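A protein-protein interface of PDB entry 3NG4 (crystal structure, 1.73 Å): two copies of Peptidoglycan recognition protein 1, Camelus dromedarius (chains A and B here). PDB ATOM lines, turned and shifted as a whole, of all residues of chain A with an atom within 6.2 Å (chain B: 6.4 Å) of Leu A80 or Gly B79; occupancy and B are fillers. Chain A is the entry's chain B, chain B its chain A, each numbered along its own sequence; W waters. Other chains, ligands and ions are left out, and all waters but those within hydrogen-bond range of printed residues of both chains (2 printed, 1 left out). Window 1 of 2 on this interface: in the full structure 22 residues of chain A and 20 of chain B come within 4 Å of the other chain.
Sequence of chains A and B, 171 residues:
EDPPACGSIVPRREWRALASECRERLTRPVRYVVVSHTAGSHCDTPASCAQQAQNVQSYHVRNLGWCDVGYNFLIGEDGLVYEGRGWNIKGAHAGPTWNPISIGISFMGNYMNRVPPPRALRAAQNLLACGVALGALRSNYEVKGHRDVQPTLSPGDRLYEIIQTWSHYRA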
ATOM      1  N   SER A   8     -24.990  32.119 -18.786  1.00  0.00           N
ATOM      2  CA  SER A   8     -24.511  31.234 -17.713  1.00  0.00           C
ATOM      3  C   SER A   8     -25.424  30.016 -17.532  1.00  0.00           C
ATOM      4  O   SER A   8     -25.742  29.616 -16.408  1.00  0.00           O
ATOM      5  CB  SER A   8     -24.335  32.003 -16.396  1.00  0.00           C
ATOM      6  OG  SER A   8     -23.386  33.046 -16.537  1.00  0.00           O
ATOM      7  N   VAL A  10     -26.782  26.243 -17.364  1.00  0.00           N
ATOM      8  CA  VAL A  10     -26.288  24.977 -16.895  1.00  0.00           C
ATOM      9  C   VAL A  10     -26.605  23.998 -18.050  1.00  0.00           C
ATOM     10  O   VAL A  10     -27.763  23.796 -18.398  1.00  0.00           O
ATOM     11  CB  VAL A  10     -27.061  24.499 -15.638  1.00  0.00           C
ATOM     12  CG1 VAL A  10     -26.656  23.069 -15.262  1.00  0.00           C
ATOM     13  CG2 VAL A  10     -26.811  25.449 -14.454  1.00  0.00           C
ATOM     14  N   THR A  45     -30.408  25.672  -4.555  1.00  0.00           N
ATOM     15  CA  THR A  45     -28.973  25.437  -4.655  1.00  0.00           C
ATOM     16  C   THR A  45     -28.711  24.775  -6.005  1.00  0.00           C
ATOM     17  O   THR A  45     -29.548  24.080  -6.504  1.00  0.00           O
ATOM     18  CB  THR A  45     -28.465  24.514  -3.553  1.00  0.00           C
ATOM     19  OG1 THR A  45     -28.951  23.186  -3.725  1.00  0.00           O
ATOM     20  CG2 THR A  45     -28.859  25.030  -2.187  1.00  0.00           C
ATOM     21  N   PRO A  46     -27.498  24.942  -6.552  1.00  0.00           N
ATOM     22  CA  PRO A  46     -27.198  24.226  -7.798  1.00  0.00           C
ATOM     23  C   PRO A  46     -27.500  22.734  -7.704  1.00  0.00           C
ATOM     24  O   PRO A  46     -28.033  22.118  -8.632  1.00  0.00           O
ATOM     25  CB  PRO A  46     -25.678  24.496  -8.003  1.00  0.00           C
ATOM     26  CG  PRO A  46     -25.477  25.844  -7.300  1.00  0.00           C
ATOM     27  CD  PRO A  46     -26.376  25.780  -6.072  1.00  0.00           C
ATOM     28  N   LEU A  74     -35.244  26.342 -18.062  1.00  0.00           N
ATOM     29  CA  LEU A  74     -35.803  26.346 -16.717  1.00  0.00           C
ATOM     30  C   LEU A  74     -35.017  27.318 -15.833  1.00  0.00           C
ATOM     31  O   LEU A  74     -33.864  27.444 -16.002  1.00  0.00           O
ATOM     32  CB  LEU A  74     -35.785  24.978 -16.073  1.00  0.00           C
ATOM     33  CG  LEU A  74     -36.569  23.942 -16.850  1.00  0.00           C
ATOM     34  CD1 LEU A  74     -35.731  23.184 -17.793  1.00  0.00           C
ATOM     35  CD2 LEU A  74     -37.371  23.007 -16.058  1.00  0.00           C
ATOM     36  N   ILE A  75     -35.702  27.964 -14.911  1.00  0.00           N
ATOM     37  CA  ILE A  75     -35.072  28.892 -14.021  1.00  0.00           C
ATOM     38  C   ILE A  75     -35.188  28.435 -12.588  1.00  0.00           C
ATOM     39  O   ILE A  75     -36.249  28.226 -12.088  1.00  0.00           O
ATOM     40  CB  ILE A  75     -35.682  30.267 -14.128  1.00  0.00           C
ATOM     41  CG1 ILE A  75     -35.887  30.658 -15.573  1.00  0.00           C
ATOM     42  CG2 ILE A  75     -34.833  31.227 -13.495  1.00  0.00           C
ATOM     43  CD1 ILE A  75     -34.649  30.959 -16.245  1.00  0.00           C
ATOM     44  N   GLY A  76     -34.049  28.294 -11.943  1.00  0.00           N
ATOM     45  CA  GLY A  76     -34.070  27.895 -10.527  1.00  0.00           C
ATOM     46  C   GLY A  76     -33.956  29.048  -9.564  1.00  0.00           C
ATOM     47  O   GLY A  76     -33.448  30.118  -9.889  1.00  0.00           O
ATOM     48  N   GLU A  77     -34.457  28.857  -8.333  1.00  0.00           N
ATOM     49  CA  GLU A  77     -34.294  29.887  -7.320  1.00  0.00           C
ATOM     50  C   GLU A  77     -32.837  29.914  -6.804  1.00  0.00           C
ATOM     51  O   GLU A  77     -32.505  30.728  -5.938  1.00  0.00           O
ATOM     52  CB  GLU A  77     -35.278  29.608  -6.137  1.00  0.00           C
ATOM     53  CG  GLU A  77     -36.672  29.916  -6.577  1.00  0.00           C
ATOM     54  CD  GLU A  77     -37.684  29.821  -5.402  1.00  0.00           C
ATOM     55  OE1 GLU A  77     -37.264  29.875  -4.277  1.00  0.00           O
ATOM     56  OE2 GLU A  77     -38.873  29.662  -5.665  1.00  0.00           O
ATOM     57  N   ASP A  78     -31.975  29.111  -7.413  1.00  0.00           N
ATOM     58  CA  ASP A  78     -30.498  29.192  -7.135  1.00  0.00           C
ATOM     59  C   ASP A  78     -29.937  30.301  -7.986  1.00  0.00           C
ATOM     60  O   ASP A  78     -28.769  30.579  -7.964  1.00  0.00           O
ATOM     61  CB  ASP A  78     -29.807  27.867  -7.415  1.00  0.00           C
ATOM     62  CG  ASP A  78     -29.950  27.423  -8.865  1.00  0.00           C
ATOM     63  OD1 ASP A  78     -30.786  27.994  -9.613  1.00  0.00           O
ATOM     64  OD2 ASP A  78     -29.295  26.462  -9.217  1.00  0.00           O
ATOM     65  N   GLY A  79     -30.798  30.926  -8.794  1.00  0.00           N
ATOM     66  CA  GLY A  79     -30.360  31.957  -9.665  1.00  0.00           C
ATOM     67  C   GLY A  79     -29.635  31.499 -10.935  1.00  0.00           C
ATOM     68  O   GLY A  79     -28.966  32.284 -11.592  1.00  0.00           O
ATOM     69  N   LEU A  80     -29.824  30.238 -11.277  1.00  0.00           N
ATOM     70  CA  LEU A  80     -29.248  29.697 -12.486  1.00  0.00           C
ATOM     71  C   LEU A  80     -30.302  29.266 -13.483  1.00  0.00           C
ATOM     72  O   LEU A  80     -31.359  28.900 -13.136  1.00  0.00           O
ATOM     73  CB  LEU A  80     -28.318  28.507 -12.258  1.00  0.00           C
ATOM     74  CG  LEU A  80     -27.178  28.682 -11.279  1.00  0.00           C
ATOM     75  CD1 LEU A  80     -26.324  27.449 -11.026  1.00  0.00           C
ATOM     76  CD2 LEU A  80     -26.372  29.723 -11.772  1.00  0.00           C
ATOM     77  N   VAL A  81     -29.911  29.300 -14.736  1.00  0.00           N
ATOM     78  CA  VAL A  81     -30.760  28.882 -15.818  1.00  0.00           C
ATOM     79  C   VAL A  81     -30.324  27.496 -16.212  1.00  0.00           C
ATOM     80  O   VAL A  81     -29.166  27.276 -16.341  1.00  0.00           O
ATOM     81  CB  VAL A  81     -30.591  29.770 -17.049  1.00  0.00           C
ATOM     82  CG1 VAL A  81     -31.382  29.271 -18.152  1.00  0.00           C
ATOM     83  CG2 VAL A  81     -31.026  31.147 -16.753  1.00  0.00           C
ATOM     84  N   TYR A  82     -31.294  26.604 -16.393  1.00  0.00           N
ATOM     85  CA  TYR A  82     -31.092  25.220 -16.805  1.00  0.00           C
ATOM     86  C   TYR A  82     -31.451  25.014 -18.270  1.00  0.00           C
ATOM     87  O   TYR A  82     -32.459  25.362 -18.679  1.00  0.00           O
ATOM     88  CB  TYR A  82     -31.857  24.262 -15.886  1.00  0.00           C
ATOM     89  CG  TYR A  82     -31.237  24.323 -14.525  1.00  0.00           C
ATOM     90  CD1 TYR A  82     -30.279  23.429 -14.174  1.00  0.00           C
ATOM     91  CD2 TYR A  82     -31.455  25.382 -13.702  1.00  0.00           C
ATOM     92  CE1 TYR A  82     -29.656  23.508 -13.011  1.00  0.00           C
ATOM     93  CE2 TYR A  82     -30.783  25.483 -12.522  1.00  0.00           C
ATOM     94  CZ  TYR A  82     -29.873  24.538 -12.177  1.00  0.00           C
ATOM     95  OH  TYR A  82     -29.217  24.567 -11.023  1.00  0.00           O
ATOM     96  N   MET A 108     -38.935  27.147 -11.836  1.00  0.00           N
ATOM     97  CA  MET A 108     -39.151  25.882 -11.151  1.00  0.00           C
ATOM     98  C   MET A 108     -39.705  26.165  -9.775  1.00  0.00           C
ATOM     99  O   MET A 108     -38.987  26.424  -8.832  1.00  0.00           O
ATOM    100  CB  MET A 108     -37.831  25.054 -11.049  1.00  0.00           C
ATOM    101  CG  MET A 108     -37.349  24.613 -12.376  1.00  0.00           C
ATOM    102  SD  MET A 108     -36.033  23.376 -12.306  1.00  0.00           S
ATOM    103  CE  MET A 108     -34.616  24.468 -11.925  1.00  0.00           C
ATOM    104  N   ARG A 119     -32.563  36.863  -7.681  1.00  0.00           N
ATOM    105  CA  ARG A 119     -31.609  36.168  -8.504  1.00  0.00           C
ATOM    106  C   ARG A 119     -32.218  35.335  -9.588  1.00  0.00           C
ATOM    107  O   ARG A 119     -31.635  35.191 -10.683  1.00  0.00           O
ATOM    108  CB  ARG A 119     -30.632  35.297  -7.615  1.00  0.00           C
ATOM    109  CG  ARG A 119     -31.307  34.170  -6.989  1.00  0.00           C
ATOM    110  CD  ARG A 119     -30.281  33.445  -5.974  1.00  0.00           C
ATOM    111  NE  ARG A 119     -31.071  32.641  -5.100  1.00  0.00           N
ATOM    112  CZ  ARG A 119     -31.466  32.978  -3.876  1.00  0.00           C
ATOM    113  NH1 ARG A 119     -31.017  34.092  -3.280  1.00  0.00           N
ATOM    114  NH2 ARG A 119     -32.197  32.134  -3.222  1.00  0.00           N
ATOM    115  N   ALA A 120     -33.424  34.803  -9.359  1.00  0.00           N
ATOM    116  CA  ALA A 120     -34.065  33.978 -10.371  1.00  0.00           C
ATOM    117  C   ALA A 120     -34.633  34.878 -11.485  1.00  0.00           C
ATOM    118  O   ALA A 120     -34.525  34.552 -12.666  1.00  0.00           O
ATOM    119  CB  ALA A 120     -35.246  33.146  -9.707  1.00  0.00           C
ATOM    120  N   ALA A 123     -31.779  36.015 -13.558  1.00  0.00           N
ATOM    121  CA  ALA A 123     -31.310  34.947 -14.394  1.00  0.00           C
ATOM    122  C   ALA A 123     -32.111  34.932 -15.670  1.00  0.00           C
ATOM    123  O   ALA A 123     -31.595  34.737 -16.740  1.00  0.00           O
ATOM    124  CB  ALA A 123     -31.366  33.596 -13.671  1.00  0.00           C
ATOM    125  N   CYS B  43     -17.883  28.349  -1.360  1.00  0.00           N
ATOM    126  CA  CYS B  43     -19.284  28.300  -0.921  1.00  0.00           C
ATOM    127  C   CYS B  43     -20.020  27.818  -2.151  1.00  0.00           C
ATOM    128  O   CYS B  43     -19.615  28.157  -3.265  1.00  0.00           O
ATOM    129  CB  CYS B  43     -19.753  29.678  -0.607  1.00  0.00           C
ATOM    130  SG  CYS B  43     -19.314  30.879  -1.885  1.00  0.00           S
ATOM    131  N   ASP B  44     -21.124  27.091  -1.973  1.00  0.00           N
ATOM    132  CA  ASP B  44     -21.774  26.580  -3.202  1.00  0.00           C
ATOM    133  C   ASP B  44     -23.272  26.802  -3.242  1.00  0.00           C
ATOM    134  O   ASP B  44     -23.975  26.074  -3.934  1.00  0.00           O
ATOM    135  CB  ASP B  44     -21.441  25.123  -3.436  1.00  0.00           C
ATOM    136  CG  ASP B  44     -21.843  24.239  -2.302  1.00  0.00           C
ATOM    137  OD1 ASP B  44     -22.496  24.702  -1.344  1.00  0.00           O
ATOM    138  OD2 ASP B  44     -21.482  23.042  -2.385  1.00  0.00           O
ATOM    139  N   CYS B  49     -22.645  31.869  -0.294  1.00  0.00           N
ATOM    140  CA  CYS B  49     -21.757  32.730  -1.057  1.00  0.00           C
ATOM    141  C   CYS B  49     -21.965  34.172  -0.811  1.00  0.00           C
ATOM    142  O   CYS B  49     -21.029  34.956  -0.895  1.00  0.00           O
ATOM    143  CB  CYS B  49     -21.862  32.458  -2.562  1.00  0.00           C
ATOM    144  SG  CYS B  49     -20.983  30.952  -3.029  1.00  0.00           S
ATOM    145  N   ILE B  75     -16.461  35.626  -7.673  1.00  0.00           N
ATOM    146  CA  ILE B  75     -17.198  34.533  -8.304  1.00  0.00           C
ATOM    147  C   ILE B  75     -17.418  33.437  -7.318  1.00  0.00           C
ATOM    148  O   ILE B  75     -16.461  32.937  -6.686  1.00  0.00           O
ATOM    149  CB  ILE B  75     -16.454  33.993  -9.530  1.00  0.00           C
ATOM    150  CG1 ILE B  75     -15.954  35.115 -10.452  1.00  0.00           C
ATOM    151  CG2 ILE B  75     -17.412  33.046 -10.291  1.00  0.00           C
ATOM    152  CD1 ILE B  75     -17.028  35.972 -11.130  1.00  0.00           C
ATOM    153  N   GLY B  76     -18.653  32.992  -7.167  1.00  0.00           N
ATOM    154  CA  GLY B  76     -18.954  31.905  -6.221  1.00  0.00           C
ATOM    155  C   GLY B  76     -19.087  30.570  -6.866  1.00  0.00           C
ATOM    156  O   GLY B  76     -19.392  30.476  -8.048  1.00  0.00           O
ATOM    157  N   GLU B  77     -18.787  29.492  -6.107  1.00  0.00           N
ATOM    158  CA  GLU B  77     -19.008  28.159  -6.641  1.00  0.00           C
ATOM    159  C   GLU B  77     -20.529  27.851  -6.781  1.00  0.00           C
ATOM    160  O   GLU B  77     -20.902  26.788  -7.207  1.00  0.00           O
ATOM    161  CB  GLU B  77     -18.308  27.086  -5.801  1.00  0.00           C
ATOM    162  CG  GLU B  77     -16.807  27.235  -5.909  1.00  0.00           C
ATOM    163  CD  GLU B  77     -16.059  26.023  -5.383  1.00  0.00           C
ATOM    164  OE1 GLU B  77     -16.640  24.917  -5.259  1.00  0.00           O
ATOM    165  OE2 GLU B  77     -14.879  26.189  -5.143  1.00  0.00           O
ATOM    166  N   ASP B  78     -21.342  28.819  -6.421  1.00  0.00           N
ATOM    167  CA  ASP B  78     -22.769  28.693  -6.577  1.00  0.00           C
ATOM    168  C   ASP B  78     -23.115  29.065  -8.034  1.00  0.00           C
ATOM    169  O   ASP B  78     -24.269  29.013  -8.472  1.00  0.00           O
ATOM    170  CB  ASP B  78     -23.510  29.586  -5.588  1.00  0.00           C
ATOM    171  CG  ASP B  78     -23.207  31.078  -5.747  1.00  0.00           C
ATOM    172  OD1 ASP B  78     -22.220  31.465  -6.436  1.00  0.00           O
ATOM    173  OD2 ASP B  78     -23.887  31.859  -5.073  1.00  0.00           O
ATOM    174  N   GLY B  79     -22.076  29.480  -8.786  1.00  0.00           N
ATOM    175  CA  GLY B  79     -22.238  29.908 -10.135  1.00  0.00           C
ATOM    176  C   GLY B  79     -22.744  31.344 -10.295  1.00  0.00           C
ATOM    177  O   GLY B  79     -23.105  31.764 -11.388  1.00  0.00           O
ATOM    178  N   LEU B  80     -22.673  32.120  -9.219  1.00  0.00           N
ATOM    179  CA  LEU B  80     -23.099  33.511  -9.243  1.00  0.00           C
ATOM    180  C   LEU B  80     -21.945  34.494  -9.126  1.00  0.00           C
ATOM    181  O   LEU B  80     -20.912  34.172  -8.551  1.00  0.00           O
ATOM    182  CB  LEU B  80     -24.092  33.768  -8.123  1.00  0.00           C
ATOM    183  CG  LEU B  80     -25.312  32.837  -8.111  1.00  0.00           C
ATOM    184  CD1 LEU B  80     -26.203  33.236  -6.910  1.00  0.00           C
ATOM    185  CD2 LEU B  80     -26.130  33.010  -9.425  1.00  0.00           C
ATOM    186  N   VAL B  81     -22.133  35.641  -9.739  1.00  0.00           N
ATOM    187  CA  VAL B  81     -21.137  36.718  -9.671  1.00  0.00           C
ATOM    188  C   VAL B  81     -21.611  37.701  -8.645  1.00  0.00           C
ATOM    189  O   VAL B  81     -22.750  38.145  -8.647  1.00  0.00           O
ATOM    190  CB  VAL B  81     -21.052  37.476 -11.035  1.00  0.00           C
ATOM    191  CG1 VAL B  81     -20.123  38.656 -10.917  1.00  0.00           C
ATOM    192  CG2 VAL B  81     -20.580  36.546 -12.142  1.00  0.00           C
ATOM    193  N   TYR B  82     -20.699  38.059  -7.744  1.00  0.00           N
ATOM    194  CA  TYR B  82     -20.981  39.051  -6.711  1.00  0.00           C
ATOM    195  C   TYR B  82     -20.346  40.425  -7.057  1.00  0.00           C
ATOM    196  O   TYR B  82     -19.176  40.509  -7.383  1.00  0.00           O
ATOM    197  CB  TYR B  82     -20.404  38.492  -5.368  1.00  0.00           C
ATOM    198  CG  TYR B  82     -21.253  37.340  -4.969  1.00  0.00           C
ATOM    199  CD1 TYR B  82     -22.356  37.517  -4.130  1.00  0.00           C
ATOM    200  CD2 TYR B  82     -21.055  36.099  -5.546  1.00  0.00           C
ATOM    201  CE1 TYR B  82     -23.216  36.481  -3.850  1.00  0.00           C
ATOM    202  CE2 TYR B  82     -21.912  35.009  -5.281  1.00  0.00           C
ATOM    203  CZ  TYR B  82     -23.011  35.249  -4.428  1.00  0.00           C
ATOM    204  OH  TYR B  82     -23.888  34.254  -4.227  1.00  0.00           O
ATOM    205  N   PRO B 117     -16.124  24.904 -10.136  1.00  0.00           N
ATOM    206  CA  PRO B 117     -16.943  24.016 -10.966  1.00  0.00           C
ATOM    207  C   PRO B 117     -17.239  24.787 -12.263  1.00  0.00           C
ATOM    208  O   PRO B 117     -17.108  25.981 -12.283  1.00  0.00           O
ATOM    209  CB  PRO B 117     -18.212  23.863 -10.102  1.00  0.00           C
ATOM    210  CG  PRO B 117     -18.270  25.168  -9.355  1.00  0.00           C
ATOM    211  CD  PRO B 117     -16.866  25.353  -8.937  1.00  0.00           C
ATOM    212  N   ARG B 119     -19.861  25.900 -13.475  1.00  0.00           N
ATOM    213  CA  ARG B 119     -20.766  27.032 -13.332  1.00  0.00           C
ATOM    214  C   ARG B 119     -20.042  28.302 -12.874  1.00  0.00           C
ATOM    215  O   ARG B 119     -20.430  29.401 -13.262  1.00  0.00           O
ATOM    216  CB  ARG B 119     -21.915  26.683 -12.325  1.00  0.00           C
ATOM    217  CG  ARG B 119     -21.522  26.408 -10.914  1.00  0.00           C
ATOM    218  CD  ARG B 119     -22.756  25.786 -10.100  1.00  0.00           C
ATOM    219  NE  ARG B 119     -22.242  25.274  -8.855  1.00  0.00           N
ATOM    220  CZ  ARG B 119     -21.929  24.010  -8.639  1.00  0.00           C
ATOM    221  NH1 ARG B 119     -22.257  23.055  -9.555  1.00  0.00           N
ATOM    222  NH2 ARG B 119     -21.407  23.695  -7.496  1.00  0.00           N
ATOM    223  N   ALA B 120     -18.975  28.142 -12.063  1.00  0.00           N
ATOM    224  CA  ALA B 120     -18.230  29.367 -11.634  1.00  0.00           C
ATOM    225  C   ALA B 120     -17.460  29.898 -12.859  1.00  0.00           C
ATOM    226  O   ALA B 120     -17.426  31.103 -13.104  1.00  0.00           O
ATOM    227  CB  ALA B 120     -17.262  28.973 -10.488  1.00  0.00           C
ATOM    228  N   ARG B 122     -18.162  29.555 -16.070  1.00  0.00           N
ATOM    229  CA  ARG B 122     -19.116  30.195 -16.978  1.00  0.00           C
ATOM    230  C   ARG B 122     -19.476  31.574 -16.554  1.00  0.00           C
ATOM    231  O   ARG B 122     -19.536  32.482 -17.385  1.00  0.00           O
ATOM    232  CB  ARG B 122     -20.411  29.381 -17.111  1.00  0.00           C
ATOM    233  CG  ARG B 122     -20.266  28.155 -18.030  1.00  0.00           C
ATOM    234  CD  ARG B 122     -21.668  27.578 -18.272  1.00  0.00           C
ATOM    235  NE  ARG B 122     -22.352  27.199 -17.039  1.00  0.00           N
ATOM    236  CZ  ARG B 122     -22.264  26.004 -16.463  1.00  0.00           C
ATOM    237  NH1 ARG B 122     -23.000  25.741 -15.372  1.00  0.00           N
ATOM    238  NH2 ARG B 122     -21.500  25.053 -16.984  1.00  0.00           N
ATOM    239  N   ALA B 123     -19.758  31.747 -15.260  1.00  0.00           N
ATOM    240  CA  ALA B 123     -20.191  33.025 -14.724  1.00  0.00           C
ATOM    241  C   ALA B 123     -19.119  34.068 -14.956  1.00  0.00           C
ATOM    242  O   ALA B 123     -19.415  35.206 -15.376  1.00  0.00           O
ATOM    243  CB  ALA B 123     -20.485  32.927 -13.229  1.00  0.00           C
HETATM  244  O   HOH W   1     -26.714  29.042  -7.132  1.00  0.00           O
HETATM  245  O   HOH W   2     -24.374  27.979 -15.012  1.00  0.00           O
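Among the printed residues, merely in contact across the chains: Pro A46 with Asp B44 (3.2 Å), Pro A46 with Asp B78 (3.6 Å), Pro A46 with Arg B119 (3.6 Å), Leu A80 with Asp B78 (3.6 Å), Gly A79 with Leu B80 (3.6 Å), Ser A8 with Ala B123 (3.7 Å), Val A10 with Arg B122 (3.7 Å), Asp A78 with Leu B80 (3.8 Å), Leu A80 with Gly B79 (3.9 Å) and Ser A8 with Arg B122 (3.98 Å).
Water W2 bridges the backbone carbonyl oxygen of Ser A8 and the guanidinium group of Arg B122. Water W1 lies within hydrogen-bond range of O of Asp A78 (2.7 Å) and O of Asp B78 (2.8 Å).
OD2 of Asp A78 lies within hydrogen-bond range of OH of Tyr A82, 2.6 Å away. The side-chain sulfur of Cys B43 forms a disulfide with the side-chain sulfur of Cys B49, 2.0 Å away. NE of Arg B119 sits at hydrogen-bond distance from O of Glu B77 (2.6 Å). The side-chain carboxylate (OD2) of Asp B78 lies within hydrogen-bond range of the side-chain hydroxyl (OH) of Tyr B82 (2.5 Å). The side-chain carboxylate (OD1) of Asp A78 sits at hydrogen-bond distance from the backbone NH (N) of Leu A80 (3.0 Å). The backbone NH (N) of Val A10 sits at hydrogen-bond distance from the backbone carbonyl oxygen (O) of Val A81 (2.8 Å).
Of the printed residues of chain B, Pro A46 touches Asp B44, Asp B78 and Arg B119. Of the printed residues of chain B, Asp A78 touches Leu B80. Leu A80 touches two residues of chain B. Pro B117 touches none of the printed residues of chain A. Of the printed residues of chain A, Ala B123 touches Ser A8. The nearest residue of chain A that does not touch Gly B79 is Ser A8 (5.2 Å). The nearest printed residue of chain B that does not touch Gly A79 is Gly B79 (5.9 Å).
Of the 16 printed residues of chain B, 7 touch a printed residue of chain A. Printed residues of chain B that touch a printed residue of chain A: Asp B44, Asp B78, Gly B79, Leu B80, Arg B119, Arg B122 and Ala B123. Hydrophobic or aromatic side chains of chain B that line the printed part of chain A: Leu B80. Of the 17 printed residues of chain A, 6 touch a printed residue of chain B. Hydrophobic or aromatic side chains of chain A within 4 Å of the printed part of chain B: Val A10, Pro A46 and Leu A80. Among the printed residues, 10 pairs touch across the chains. Among the printed residues, no Asp or Glu carboxylate lies within 4 Å of a Lys or Arg side-chain nitrogen of the other chain.
Asp A78 touches Leu B80, and with the chains exchanged Leu A80 touches Asp B78. Gly A79 touches Leu B80, and with the chains exchanged Leu A80 touches Gly B79. Of the 10 pairs that touch across the chains among the printed residues, 4 have their exchanged pair printed and touching as well.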
